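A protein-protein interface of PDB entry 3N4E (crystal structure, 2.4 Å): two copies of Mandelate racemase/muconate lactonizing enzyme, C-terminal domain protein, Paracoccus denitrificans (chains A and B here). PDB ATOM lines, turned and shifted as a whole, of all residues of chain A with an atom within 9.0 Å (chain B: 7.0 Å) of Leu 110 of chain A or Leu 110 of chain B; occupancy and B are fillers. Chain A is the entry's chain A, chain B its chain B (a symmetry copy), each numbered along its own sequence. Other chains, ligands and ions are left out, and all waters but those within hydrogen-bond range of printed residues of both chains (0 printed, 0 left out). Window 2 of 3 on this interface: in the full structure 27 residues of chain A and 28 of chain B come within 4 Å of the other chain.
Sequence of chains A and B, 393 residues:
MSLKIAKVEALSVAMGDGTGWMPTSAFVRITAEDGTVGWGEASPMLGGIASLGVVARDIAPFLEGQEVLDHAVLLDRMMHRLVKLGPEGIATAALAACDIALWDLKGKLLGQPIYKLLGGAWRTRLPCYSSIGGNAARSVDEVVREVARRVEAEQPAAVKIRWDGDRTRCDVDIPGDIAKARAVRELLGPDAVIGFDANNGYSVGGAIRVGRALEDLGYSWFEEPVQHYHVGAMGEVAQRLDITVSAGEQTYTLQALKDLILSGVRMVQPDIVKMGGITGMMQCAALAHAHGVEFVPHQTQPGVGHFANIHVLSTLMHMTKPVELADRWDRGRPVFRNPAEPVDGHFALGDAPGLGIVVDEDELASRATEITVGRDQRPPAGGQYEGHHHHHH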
ATOM      1  N   SER A   2      -3.935 -24.283 -33.174  1.00  0.00           N
ATOM      2  CA  SER A   2      -4.666 -23.444 -32.183  1.00  0.00           C
ATOM      3  C   SER A   2      -4.656 -21.969 -32.619  1.00  0.00           C
ATOM      4  O   SER A   2      -4.375 -21.670 -33.789  1.00  0.00           O
ATOM      5  CB  SER A   2      -4.078 -23.642 -30.773  1.00  0.00           C
ATOM      6  OG  SER A   2      -4.836 -22.977 -29.766  1.00  0.00           O
ATOM      7  N   LEU A   3      -4.952 -21.068 -31.677  1.00  0.00           N
ATOM      8  CA  LEU A   3      -5.239 -19.648 -31.940  1.00  0.00           C
ATOM      9  C   LEU A   3      -4.088 -18.783 -32.516  1.00  0.00           C
ATOM     10  O   LEU A   3      -2.974 -18.776 -31.996  1.00  0.00           O
ATOM     11  CB  LEU A   3      -5.784 -19.015 -30.655  1.00  0.00           C
ATOM     12  CG  LEU A   3      -6.420 -17.631 -30.715  1.00  0.00           C
ATOM     13  CD1 LEU A   3      -7.754 -17.714 -31.436  1.00  0.00           C
ATOM     14  CD2 LEU A   3      -6.590 -17.069 -29.308  1.00  0.00           C
ATOM     15  N   ASP A  34      -9.902 -15.006 -33.361  1.00  0.00           N
ATOM     16  CA  ASP A  34     -11.277 -15.135 -32.866  1.00  0.00           C
ATOM     17  C   ASP A  34     -11.790 -13.817 -32.299  1.00  0.00           C
ATOM     18  O   ASP A  34     -12.825 -13.771 -31.629  1.00  0.00           O
ATOM     19  CB  ASP A  34     -11.417 -16.284 -31.852  1.00  0.00           C
ATOM     20  CG  ASP A  34     -10.648 -16.052 -30.563  1.00  0.00           C
ATOM     21  OD1 ASP A  34      -9.908 -15.052 -30.427  1.00  0.00           O
ATOM     22  OD2 ASP A  34     -10.775 -16.907 -29.670  1.00  0.00           O
ATOM     23  N   THR A  36     -10.514 -11.901 -29.984  1.00  0.00           N
ATOM     24  CA  THR A  36     -10.111 -11.566 -28.625  1.00  0.00           C
ATOM     25  C   THR A  36      -8.911 -10.617 -28.681  1.00  0.00           C
ATOM     26  O   THR A  36      -8.148 -10.615 -29.657  1.00  0.00           O
ATOM     27  CB  THR A  36      -9.814 -12.807 -27.764  1.00  0.00           C
ATOM     28  OG1 THR A  36      -8.852 -13.629 -28.432  1.00  0.00           O
ATOM     29  CG2 THR A  36     -11.083 -13.613 -27.538  1.00  0.00           C
ATOM     30  N   VAL A  68      -0.370 -17.480 -30.781  1.00  0.00           N
ATOM     31  CA  VAL A  68      -0.341 -16.713 -29.526  1.00  0.00           C
ATOM     32  C   VAL A  68       0.511 -17.402 -28.447  1.00  0.00           C
ATOM     33  O   VAL A  68       1.274 -16.748 -27.729  1.00  0.00           O
ATOM     34  CB  VAL A  68      -1.780 -16.483 -28.949  1.00  0.00           C
ATOM     35  CG1 VAL A  68      -1.728 -15.763 -27.591  1.00  0.00           C
ATOM     36  CG2 VAL A  68      -2.637 -15.708 -29.920  1.00  0.00           C
ATOM     37  N   LEU A  69       0.371 -18.721 -28.340  1.00  0.00           N
ATOM     38  CA  LEU A  69       1.022 -19.485 -27.281  1.00  0.00           C
ATOM     39  C   LEU A  69       2.515 -19.640 -27.500  1.00  0.00           C
ATOM     40  O   LEU A  69       3.227 -20.122 -26.611  1.00  0.00           O
ATOM     41  CB  LEU A  69       0.359 -20.858 -27.123  1.00  0.00           C
ATOM     42  CG  LEU A  69      -1.082 -20.836 -26.586  1.00  0.00           C
ATOM     43  CD1 LEU A  69      -1.711 -22.235 -26.602  1.00  0.00           C
ATOM     44  CD2 LEU A  69      -1.132 -20.201 -25.188  1.00  0.00           C
ATOM     45  N   HIS A  71       4.582 -17.289 -27.598  1.00  0.00           N
ATOM     46  CA  HIS A  71       5.089 -15.974 -27.207  1.00  0.00           C
ATOM     47  C   HIS A  71       6.592 -15.918 -26.897  1.00  0.00           C
ATOM     48  O   HIS A  71       7.289 -15.028 -27.384  1.00  0.00           O
ATOM     49  CB  HIS A  71       4.256 -15.369 -26.067  1.00  0.00           C
ATOM     50  CG  HIS A  71       4.287 -16.157 -24.803  1.00  0.00           C
ATOM     51  ND1 HIS A  71       5.220 -15.936 -23.813  1.00  0.00           N
ATOM     52  CD2 HIS A  71       3.493 -17.157 -24.355  1.00  0.00           C
ATOM     53  CE1 HIS A  71       5.009 -16.773 -22.812  1.00  0.00           C
ATOM     54  NE2 HIS A  71       3.963 -17.523 -23.115  1.00  0.00           N
ATOM     55  N   LEU A 102       0.507 -10.538 -25.436  1.00  0.00           N
ATOM     56  CA  LEU A 102       0.365 -11.982 -25.669  1.00  0.00           C
ATOM     57  C   LEU A 102      -0.005 -12.752 -24.399  1.00  0.00           C
ATOM     58  O   LEU A 102      -0.783 -13.702 -24.461  1.00  0.00           O
ATOM     59  CB  LEU A 102       1.624 -12.579 -26.339  1.00  0.00           C
ATOM     60  CG  LEU A 102       1.929 -12.077 -27.765  1.00  0.00           C
ATOM     61  CD1 LEU A 102       3.321 -12.492 -28.251  1.00  0.00           C
ATOM     62  CD2 LEU A 102       0.862 -12.521 -28.773  1.00  0.00           C
ATOM     63  N   TRP A 103       0.529 -12.343 -23.251  1.00  0.00           N
ATOM     64  CA  TRP A 103       0.119 -12.937 -21.970  1.00  0.00           C
ATOM     65  C   TRP A 103      -1.353 -12.668 -21.649  1.00  0.00           C
ATOM     66  O   TRP A 103      -2.052 -13.547 -21.142  1.00  0.00           O
ATOM     67  CB  TRP A 103       1.010 -12.462 -20.817  1.00  0.00           C
ATOM     68  CG  TRP A 103       2.204 -13.329 -20.620  1.00  0.00           C
ATOM     69  CD1 TRP A 103       3.470 -13.101 -21.081  1.00  0.00           C
ATOM     70  CD2 TRP A 103       2.244 -14.586 -19.934  1.00  0.00           C
ATOM     71  NE1 TRP A 103       4.303 -14.141 -20.711  1.00  0.00           N
ATOM     72  CE2 TRP A 103       3.574 -15.066 -20.015  1.00  0.00           C
ATOM     73  CE3 TRP A 103       1.288 -15.354 -19.264  1.00  0.00           C
ATOM     74  CZ2 TRP A 103       3.972 -16.266 -19.433  1.00  0.00           C
ATOM     75  CZ3 TRP A 103       1.677 -16.559 -18.695  1.00  0.00           C
ATOM     76  CH2 TRP A 103       3.009 -17.000 -18.774  1.00  0.00           C
ATOM     77  N   ASP A 104      -1.815 -11.465 -21.969  1.00  0.00           N
ATOM     78  CA  ASP A 104      -3.208 -11.099 -21.768  1.00  0.00           C
ATOM     79  C   ASP A 104      -4.092 -12.044 -22.585  1.00  0.00           C
ATOM     80  O   ASP A 104      -5.030 -12.654 -22.049  1.00  0.00           O
ATOM     81  CB  ASP A 104      -3.433  -9.622 -22.161  1.00  0.00           C
ATOM     82  CG  ASP A 104      -4.679  -9.027 -21.528  1.00  0.00           C
ATOM     83  OD1 ASP A 104      -5.123  -9.525 -20.476  1.00  0.00           O
ATOM     84  OD2 ASP A 104      -5.218  -8.046 -22.076  1.00  0.00           O
ATOM     85  N   LEU A 105      -3.745 -12.190 -23.867  1.00  0.00           N
ATOM     86  CA  LEU A 105      -4.395 -13.110 -24.788  1.00  0.00           C
ATOM     87  C   LEU A 105      -4.333 -14.550 -24.311  1.00  0.00           C
ATOM     88  O   LEU A 105      -5.368 -15.230 -24.275  1.00  0.00           O
ATOM     89  CB  LEU A 105      -3.773 -13.005 -26.185  1.00  0.00           C
ATOM     90  CG  LEU A 105      -4.275 -11.859 -27.058  1.00  0.00           C
ATOM     91  CD1 LEU A 105      -3.501 -11.824 -28.363  1.00  0.00           C
ATOM     92  CD2 LEU A 105      -5.790 -11.965 -27.313  1.00  0.00           C
ATOM     93  N   LYS A 106      -3.124 -15.010 -23.961  1.00  0.00           N
ATOM     94  CA  LYS A 106      -2.895 -16.367 -23.428  1.00  0.00           C
ATOM     95  C   LYS A 106      -3.875 -16.659 -22.282  1.00  0.00           C
ATOM     96  O   LYS A 106      -4.512 -17.707 -22.246  1.00  0.00           O
ATOM     97  CB  LYS A 106      -1.456 -16.475 -22.941  1.00  0.00           C
ATOM     98  CG  LYS A 106      -1.073 -17.771 -22.293  1.00  0.00           C
ATOM     99  CD  LYS A 106       0.447 -17.851 -22.156  1.00  0.00           C
ATOM    100  CE  LYS A 106       0.874 -19.056 -21.322  1.00  0.00           C
ATOM    101  NZ  LYS A 106       2.360 -19.223 -21.268  1.00  0.00           N
ATOM    102  N   GLY A 107      -4.000 -15.698 -21.370  1.00  0.00           N
ATOM    103  CA  GLY A 107      -4.850 -15.845 -20.189  1.00  0.00           C
ATOM    104  C   GLY A 107      -6.328 -15.844 -20.522  1.00  0.00           C
ATOM    105  O   GLY A 107      -7.107 -16.580 -19.907  1.00  0.00           O
ATOM    106  N   LYS A 108      -6.711 -15.012 -21.487  1.00  0.00           N
ATOM    107  CA  LYS A 108      -8.082 -14.962 -21.951  1.00  0.00           C
ATOM    108  C   LYS A 108      -8.441 -16.250 -22.666  1.00  0.00           C
ATOM    109  O   LYS A 108      -9.505 -16.808 -22.405  1.00  0.00           O
ATOM    110  CB  LYS A 108      -8.331 -13.737 -22.848  1.00  0.00           C
ATOM    111  CG  LYS A 108      -8.461 -12.452 -22.059  1.00  0.00           C
ATOM    112  CD  LYS A 108      -8.756 -11.263 -22.939  1.00  0.00           C
ATOM    113  CE  LYS A 108      -8.651  -9.972 -22.138  1.00  0.00           C
ATOM    114  NZ  LYS A 108      -8.770  -8.762 -23.016  1.00  0.00           N
ATOM    115  N   LEU A 109      -7.552 -16.728 -23.541  1.00  0.00           N
ATOM    116  CA  LEU A 109      -7.742 -18.003 -24.252  1.00  0.00           C
ATOM    117  C   LEU A 109      -7.882 -19.191 -23.304  1.00  0.00           C
ATOM    118  O   LEU A 109      -8.738 -20.057 -23.499  1.00  0.00           O
ATOM    119  CB  LEU A 109      -6.584 -18.259 -25.241  1.00  0.00           C
ATOM    120  CG  LEU A 109      -6.234 -19.694 -25.713  1.00  0.00           C
ATOM    121  CD1 LEU A 109      -7.325 -20.360 -26.574  1.00  0.00           C
ATOM    122  CD2 LEU A 109      -4.921 -19.706 -26.482  1.00  0.00           C
ATOM    123  N   LEU A 110      -7.023 -19.226 -22.289  1.00  0.00           N
ATOM    124  CA  LEU A 110      -6.951 -20.354 -21.369  1.00  0.00           C
ATOM    125  C   LEU A 110      -7.941 -20.239 -20.207  1.00  0.00           C
ATOM    126  O   LEU A 110      -8.127 -21.190 -19.449  1.00  0.00           O
ATOM    127  CB  LEU A 110      -5.510 -20.530 -20.862  1.00  0.00           C
ATOM    128  CG  LEU A 110      -4.464 -20.961 -21.907  1.00  0.00           C
ATOM    129  CD1 LEU A 110      -3.121 -21.212 -21.292  1.00  0.00           C
ATOM    130  CD2 LEU A 110      -4.924 -22.200 -22.668  1.00  0.00           C
ATOM    131  N   GLY A 111      -8.572 -19.076 -20.072  1.00  0.00           N
ATOM    132  CA  GLY A 111      -9.580 -18.854 -19.037  1.00  0.00           C
ATOM    133  C   GLY A 111      -9.011 -18.595 -17.652  1.00  0.00           C
ATOM    134  O   GLY A 111      -9.676 -18.869 -16.665  1.00  0.00           O
ATOM    135  N   GLN A 112      -7.791 -18.065 -17.571  1.00  0.00           N
ATOM    136  CA  GLN A 112      -7.131 -17.887 -16.274  1.00  0.00           C
ATOM    137  C   GLN A 112      -6.498 -16.515 -16.081  1.00  0.00           C
ATOM    138  O   GLN A 112      -6.094 -15.873 -17.050  1.00  0.00           O
ATOM    139  CB  GLN A 112      -6.064 -18.973 -16.042  1.00  0.00           C
ATOM    140  CG  GLN A 112      -6.580 -20.414 -16.037  1.00  0.00           C
ATOM    141  CD  GLN A 112      -7.531 -20.717 -14.884  1.00  0.00           C
ATOM    142  OE1 GLN A 112      -7.544 -20.024 -13.862  1.00  0.00           O
ATOM    143  NE2 GLN A 112      -8.325 -21.767 -15.039  1.00  0.00           N
ATOM    144  N   PRO A 113      -6.428 -16.045 -14.821  1.00  0.00           N
ATOM    145  CA  PRO A 113      -5.606 -14.869 -14.619  1.00  0.00           C
ATOM    146  C   PRO A 113      -4.134 -15.244 -14.791  1.00  0.00           C
ATOM    147  O   PRO A 113      -3.752 -16.398 -14.554  1.00  0.00           O
ATOM    148  CB  PRO A 113      -5.905 -14.455 -13.175  1.00  0.00           C
ATOM    149  CG  PRO A 113      -6.508 -15.658 -12.519  1.00  0.00           C
ATOM    150  CD  PRO A 113      -7.141 -16.464 -13.597  1.00  0.00           C
ATOM    151  N   ILE A 114      -3.323 -14.281 -15.212  1.00  0.00           N
ATOM    152  CA  ILE A 114      -1.913 -14.534 -15.465  1.00  0.00           C
ATOM    153  C   ILE A 114      -1.197 -15.207 -14.294  1.00  0.00           C
ATOM    154  O   ILE A 114      -0.452 -16.187 -14.497  1.00  0.00           O
ATOM    155  CB  ILE A 114      -1.171 -13.270 -15.949  1.00  0.00           C
ATOM    156  CG1 ILE A 114      -1.654 -12.917 -17.367  1.00  0.00           C
ATOM    157  CG2 ILE A 114       0.333 -13.506 -15.953  1.00  0.00           C
ATOM    158  CD1 ILE A 114      -1.326 -11.514 -17.807  1.00  0.00           C
ATOM    159  N   LYS A 116      -2.248 -17.207 -12.121  1.00  0.00           N
ATOM    160  CA  LYS A 116      -2.634 -18.621 -12.070  1.00  0.00           C
ATOM    161  C   LYS A 116      -1.993 -19.450 -13.191  1.00  0.00           C
ATOM    162  O   LYS A 116      -1.971 -20.673 -13.129  1.00  0.00           O
ATOM    163  CB  LYS A 116      -4.157 -18.782 -12.094  1.00  0.00           C
ATOM    164  CG  LYS A 116      -4.859 -18.356 -10.810  1.00  0.00           C
ATOM    165  CD  LYS A 116      -4.922 -19.503  -9.838  1.00  0.00           C
ATOM    166  CE  LYS A 116      -5.628 -19.136  -8.530  1.00  0.00           C
ATOM    167  NZ  LYS A 116      -5.728 -20.355  -7.633  1.00  0.00           N
ATOM    168  N   LEU A 117      -1.443 -18.788 -14.203  1.00  0.00           N
ATOM    169  CA  LEU A 117      -0.654 -19.505 -15.192  1.00  0.00           C
ATOM    170  C   LEU A 117       0.785 -19.560 -14.746  1.00  0.00           C
ATOM    171  O   LEU A 117       1.534 -20.409 -15.206  1.00  0.00           O
ATOM    172  CB  LEU A 117      -0.773 -18.858 -16.564  1.00  0.00           C
ATOM    173  CG  LEU A 117      -2.196 -18.815 -17.116  1.00  0.00           C
ATOM    174  CD1 LEU A 117      -2.227 -17.994 -18.383  1.00  0.00           C
ATOM    175  CD2 LEU A 117      -2.692 -20.224 -17.372  1.00  0.00           C
ATOM    176  N   LEU A 118       1.156 -18.677 -13.817  1.00  0.00           N
ATOM    177  CA  LEU A 118       2.519 -18.597 -13.314  1.00  0.00           C
ATOM    178  C   LEU A 118       2.786 -19.438 -12.069  1.00  0.00           C
ATOM    179  O   LEU A 118       3.872 -19.307 -11.459  1.00  0.00           O
ATOM    180  CB  LEU A 118       2.886 -17.141 -13.023  1.00  0.00           C
ATOM    181  CG  LEU A 118       3.078 -16.281 -14.273  1.00  0.00           C
ATOM    182  CD1 LEU A 118       3.406 -14.835 -13.905  1.00  0.00           C
ATOM    183  CD2 LEU A 118       4.158 -16.896 -15.196  1.00  0.00           C
ATOM    184  N   PRO A 353      -9.630 -13.310 -16.365  1.00  0.00           N
ATOM    185  CA  PRO A 353      -8.691 -13.923 -17.307  1.00  0.00           C
ATOM    186  C   PRO A 353      -7.697 -12.895 -17.855  1.00  0.00           C
ATOM    187  O   PRO A 353      -8.052 -11.735 -18.034  1.00  0.00           O
ATOM    188  CB  PRO A 353      -9.598 -14.430 -18.431  1.00  0.00           C
ATOM    189  CG  PRO A 353     -10.945 -14.595 -17.800  1.00  0.00           C
ATOM    190  CD  PRO A 353     -11.037 -13.499 -16.782  1.00  0.00           C
ATOM    191  N   GLY A 354      -6.469 -13.317 -18.120  1.00  0.00           N
ATOM    192  CA  GLY A 354      -5.429 -12.402 -18.605  1.00  0.00           C
ATOM    193  C   GLY A 354      -4.945 -11.410 -17.560  1.00  0.00           C
ATOM    194  O   GLY A 354      -4.781 -11.750 -16.386  1.00  0.00           O
ATOM    195  N   LEU B  69      -3.510 -25.246  -9.877  1.00  0.00           N
ATOM    196  CA  LEU B  69      -2.842 -24.038 -10.400  1.00  0.00           C
ATOM    197  C   LEU B  69      -1.988 -23.268  -9.378  1.00  0.00           C
ATOM    198  O   LEU B  69      -1.191 -22.410  -9.759  1.00  0.00           O
ATOM    199  CB  LEU B  69      -3.846 -23.113 -11.108  1.00  0.00           C
ATOM    200  CG  LEU B  69      -4.532 -23.779 -12.313  1.00  0.00           C
ATOM    201  CD1 LEU B  69      -5.663 -22.923 -12.892  1.00  0.00           C
ATOM    202  CD2 LEU B  69      -3.524 -24.129 -13.385  1.00  0.00           C
ATOM    203  N   LEU B 105      -1.243 -32.451 -14.859  1.00  0.00           N
ATOM    204  CA  LEU B 105      -2.621 -32.116 -14.514  1.00  0.00           C
ATOM    205  C   LEU B 105      -2.997 -30.738 -15.064  1.00  0.00           C
ATOM    206  O   LEU B 105      -4.097 -30.542 -15.586  1.00  0.00           O
ATOM    207  CB  LEU B 105      -2.742 -32.119 -12.996  1.00  0.00           C
ATOM    208  CG  LEU B 105      -3.860 -32.784 -12.214  1.00  0.00           C
ATOM    209  CD1 LEU B 105      -4.503 -33.987 -12.942  1.00  0.00           C
ATOM    210  CD2 LEU B 105      -3.252 -33.201 -10.889  1.00  0.00           C
ATOM    211  N   LYS B 106      -2.070 -29.794 -14.966  1.00  0.00           N
ATOM    212  CA  LYS B 106      -2.291 -28.445 -15.472  1.00  0.00           C
ATOM    213  C   LYS B 106      -2.509 -28.458 -16.989  1.00  0.00           C
ATOM    214  O   LYS B 106      -3.407 -27.789 -17.494  1.00  0.00           O
ATOM    215  CB  LYS B 106      -1.110 -27.553 -15.081  1.00  0.00           C
ATOM    216  CG  LYS B 106      -1.156 -26.113 -15.554  1.00  0.00           C
ATOM    217  CD  LYS B 106       0.015 -25.383 -14.924  1.00  0.00           C
ATOM    218  CE  LYS B 106       0.162 -23.988 -15.427  1.00  0.00           C
ATOM    219  NZ  LYS B 106       1.454 -23.420 -14.943  1.00  0.00           N
ATOM    220  N   GLY B 107      -1.692 -29.232 -17.701  1.00  0.00           N
ATOM    221  CA  GLY B 107      -1.799 -29.324 -19.156  1.00  0.00           C
ATOM    222  C   GLY B 107      -3.114 -29.932 -19.619  1.00  0.00           C
ATOM    223  O   GLY B 107      -3.693 -29.491 -20.612  1.00  0.00           O
ATOM    224  N   LYS B 108      -3.592 -30.929 -18.880  1.00  0.00           N
ATOM    225  CA  LYS B 108      -4.864 -31.584 -19.191  1.00  0.00           C
ATOM    226  C   LYS B 108      -6.062 -30.676 -18.903  1.00  0.00           C
ATOM    227  O   LYS B 108      -7.009 -30.641 -19.684  1.00  0.00           O
ATOM    228  CB  LYS B 108      -4.991 -32.906 -18.436  1.00  0.00           C
ATOM    229  CG  LYS B 108      -4.079 -33.989 -18.956  1.00  0.00           C
ATOM    230  CD  LYS B 108      -4.102 -35.238 -18.087  1.00  0.00           C
ATOM    231  CE  LYS B 108      -3.097 -36.276 -18.573  1.00  0.00           C
ATOM    232  NZ  LYS B 108      -3.041 -37.468 -17.677  1.00  0.00           N
ATOM    233  N   LEU B 109      -6.008 -29.949 -17.788  1.00  0.00           N
ATOM    234  CA  LEU B 109      -7.052 -29.004 -17.395  1.00  0.00           C
ATOM    235  C   LEU B 109      -7.192 -27.884 -18.417  1.00  0.00           C
ATOM    236  O   LEU B 109      -8.296 -27.412 -18.686  1.00  0.00           O
ATOM    237  CB  LEU B 109      -6.745 -28.415 -16.011  1.00  0.00           C
ATOM    238  CG  LEU B 109      -7.374 -27.077 -15.567  1.00  0.00           C
ATOM    239  CD1 LEU B 109      -8.913 -27.141 -15.399  1.00  0.00           C
ATOM    240  CD2 LEU B 109      -6.726 -26.581 -14.284  1.00  0.00           C
ATOM    241  N   LEU B 110      -6.069 -27.470 -18.996  1.00  0.00           N
ATOM    242  CA  LEU B 110      -6.055 -26.340 -19.915  1.00  0.00           C
ATOM    243  C   LEU B 110      -6.101 -26.746 -21.392  1.00  0.00           C
ATOM    244  O   LEU B 110      -6.247 -25.891 -22.272  1.00  0.00           O
ATOM    245  CB  LEU B 110      -4.836 -25.456 -19.618  1.00  0.00           C
ATOM    246  CG  LEU B 110      -4.782 -24.828 -18.221  1.00  0.00           C
ATOM    247  CD1 LEU B 110      -3.464 -24.077 -17.997  1.00  0.00           C
ATOM    248  CD2 LEU B 110      -5.984 -23.912 -17.982  1.00  0.00           C
ATOM    249  N   GLY B 111      -5.959 -28.041 -21.658  1.00  0.00           N
ATOM    250  CA  GLY B 111      -6.048 -28.575 -23.018  1.00  0.00           C
ATOM    251  C   GLY B 111      -4.819 -28.306 -23.866  1.00  0.00           C
ATOM    252  O   GLY B 111      -4.913 -28.162 -25.087  1.00  0.00           O
ATOM    253  N   GLN B 112      -3.662 -28.241 -23.223  1.00  0.00           N
ATOM    254  CA  GLN B 112      -2.439 -27.869 -23.913  1.00  0.00           C
ATOM    255  C   GLN B 112      -1.263 -28.757 -23.525  1.00  0.00           C
ATOM    256  O   GLN B 112      -1.109 -29.135 -22.350  1.00  0.00           O
ATOM    257  CB  GLN B 112      -2.082 -26.397 -23.632  1.00  0.00           C
ATOM    258  CG  GLN B 112      -3.068 -25.370 -24.193  1.00  0.00           C
ATOM    259  CD  GLN B 112      -3.081 -25.326 -25.713  1.00  0.00           C
ATOM    260  OE1 GLN B 112      -2.093 -25.676 -26.369  1.00  0.00           O
ATOM    261  NE2 GLN B 112      -4.201 -24.892 -26.282  1.00  0.00           N
ATOM    262  N   PRO B 113      -0.425 -29.103 -24.515  1.00  0.00           N
ATOM    263  CA  PRO B 113       0.846 -29.775 -24.215  1.00  0.00           C
ATOM    264  C   PRO B 113       1.689 -28.855 -23.334  1.00  0.00           C
ATOM    265  O   PRO B 113       1.530 -27.639 -23.395  1.00  0.00           O
ATOM    266  CB  PRO B 113       1.494 -29.961 -25.596  1.00  0.00           C
ATOM    267  CG  PRO B 113       0.692 -29.133 -26.549  1.00  0.00           C
ATOM    268  CD  PRO B 113      -0.655 -28.923 -25.957  1.00  0.00           C
ATOM    269  N   LYS B 116       3.516 -25.828 -24.786  1.00  0.00           N
ATOM    270  CA  LYS B 116       2.576 -24.767 -25.141  1.00  0.00           C
ATOM    271  C   LYS B 116       2.189 -23.865 -23.948  1.00  0.00           C
ATOM    272  O   LYS B 116       1.647 -22.781 -24.136  1.00  0.00           O
ATOM    273  CB  LYS B 116       1.316 -25.355 -25.804  1.00  0.00           C
ATOM    274  CG  LYS B 116       1.524 -25.799 -27.255  1.00  0.00           C
ATOM    275  CD  LYS B 116       1.645 -24.616 -28.198  1.00  0.00           C
ATOM    276  CE  LYS B 116       2.057 -25.047 -29.601  1.00  0.00           C
ATOM    277  NZ  LYS B 116       2.109 -23.880 -30.561  1.00  0.00           N
ATOM    278  N   LEU B 117       2.432 -24.327 -22.727  1.00  0.00           N
ATOM    279  CA  LEU B 117       2.149 -23.528 -21.544  1.00  0.00           C
ATOM    280  C   LEU B 117       3.392 -22.740 -21.178  1.00  0.00           C
ATOM    281  O   LEU B 117       3.309 -21.737 -20.471  1.00  0.00           O
ATOM    282  CB  LEU B 117       1.662 -24.410 -20.371  1.00  0.00           C
ATOM    283  CG  LEU B 117       0.313 -25.133 -20.592  1.00  0.00           C
ATOM    284  CD1 LEU B 117      -0.009 -26.100 -19.477  1.00  0.00           C
ATOM    285  CD2 LEU B 117      -0.844 -24.152 -20.781  1.00  0.00           C
ATOM    286  N   PRO B 353      -2.196 -33.048 -24.536  1.00  0.00           N
ATOM    287  CA  PRO B 353      -2.117 -32.149 -23.388  1.00  0.00           C
ATOM    288  C   PRO B 353      -1.346 -32.751 -22.210  1.00  0.00           C
ATOM    289  O   PRO B 353      -1.329 -33.977 -22.019  1.00  0.00           O
ATOM    290  CB  PRO B 353      -3.582 -31.877 -23.047  1.00  0.00           C
ATOM    291  CG  PRO B 353      -4.322 -33.035 -23.612  1.00  0.00           C
ATOM    292  CD  PRO B 353      -3.585 -33.444 -24.838  1.00  0.00           C
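The backbone carbonyl oxygen (O) of Leu 117 of chain B sits at hydrogen-bond distance from the side-chain amino group (NZ) of Lys 106 of chain A, 2.8 Å away. NZ of Lys 106 of chain B lies within hydrogen-bond range of O of Leu 117 of chain A (3.0 Å).
NZ of Lys 106 of chain A is in hydrogen-bond range of NE2 of His 71 of chain A (3.0 Å). The backbone carbonyl oxygen (O) of Gly 107 of chain A lies within hydrogen-bond range of the backbone NH (N) of Gln 112 of chain A (2.9 Å). O of Gln 112 of chain A sits at hydrogen-bond distance from N of Gly 354 of chain A (2.8 Å). The backbone NH of Gln 112 of chain B is in hydrogen-bond range of the backbone carbonyl oxygen of Gly 107 of chain B (2.9 Å).
Leu 69 of chain A touches Lys 116 of chain B, and with the chains exchanged Lys 116 of chain A touches Leu 69 of chain B. Leu 110 of chain A touches its own counterpart, Leu 110 of chain B. Leu 110 of chain A touches Gln 112 of chain B, but with the chains exchanged Gln 112 of chain A does not touch Leu 110 of chain B (4.05 Å). Leu 110 of chain A touches Leu 117 of chain B, and with the chains exchanged Leu 117 of chain A touches Leu 110 of chain B.
Gly 107 of chain A touches none of the printed residues of chain B. Of chain B, only Leu 110, Gln 112 and Leu 117 come within 4 Å of Leu 110 of chain A. Printed residues of chain A within 4 Å of Leu 69 of chain B: Gln 112 (3.5 Å) and Lys 116 (3.7 Å). Of the printed residues of chain A, Lys 106 of chain B touches Leu 117 (3.0 Å). Leu 109 of chain B touches none of the printed residues of chain A. Of chain A, only Leu 110 (3.8 Å) and Leu 117 (3.98 Å) come within 4 Å of Leu 110 of chain B. Printed residues of chain A within 4 Å of Lys 116 of chain B: Leu 69 (3.8 Å). The nearest residue of chain B that does not touch Leu 110 of chain A is Lys 116 of chain B (5.8 Å). The nearest residue of chain A that does not touch Leu 110 of chain B is Gln 112 of chain A (4.05 Å).
Among the printed residues, merely in contact across the chains: Leu 69 of chain A with Gln 112 of chain B (3.5 Å), Leu 69 of chain A with Lys 116 of chain B (3.8 Å), Leu 110 of chain A with Leu 110 of chain B (3.8 Å), Leu 110 of chain A with Gln 112 of chain B (3.98 Å), Leu 110 of chain A with Leu 117 of chain B (3.8 Å), Gln 112 of chain A with Leu 69 of chain B (3.5 Å), Lys 116 of chain A with Leu 69 of chain B (3.7 Å) and Leu 117 of chain A with Leu 110 of chain B (3.98 Å).
Printed residues of chain B that touch a printed residue of chain A: Leu 69, Lys 106, Leu 110, Gln 112, Lys 116 and Leu 117. Hydrophobic or aromatic side chains of chain B that line the printed part of chain A: Leu 69, Leu 110 and Leu 117. Printed residues of chain A that touch a printed residue of chain B: Leu 69, Lys 106, Leu 110, Gln 112, Lys 116 and Leu 117. Hydrophobic or aromatic side chains of chain A within 4 Å of the printed part of chain B: Leu 69, Leu 110 and Leu 117. Along chain A the printed residues that touch a printed residue of chain B span positions 69 to 117.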
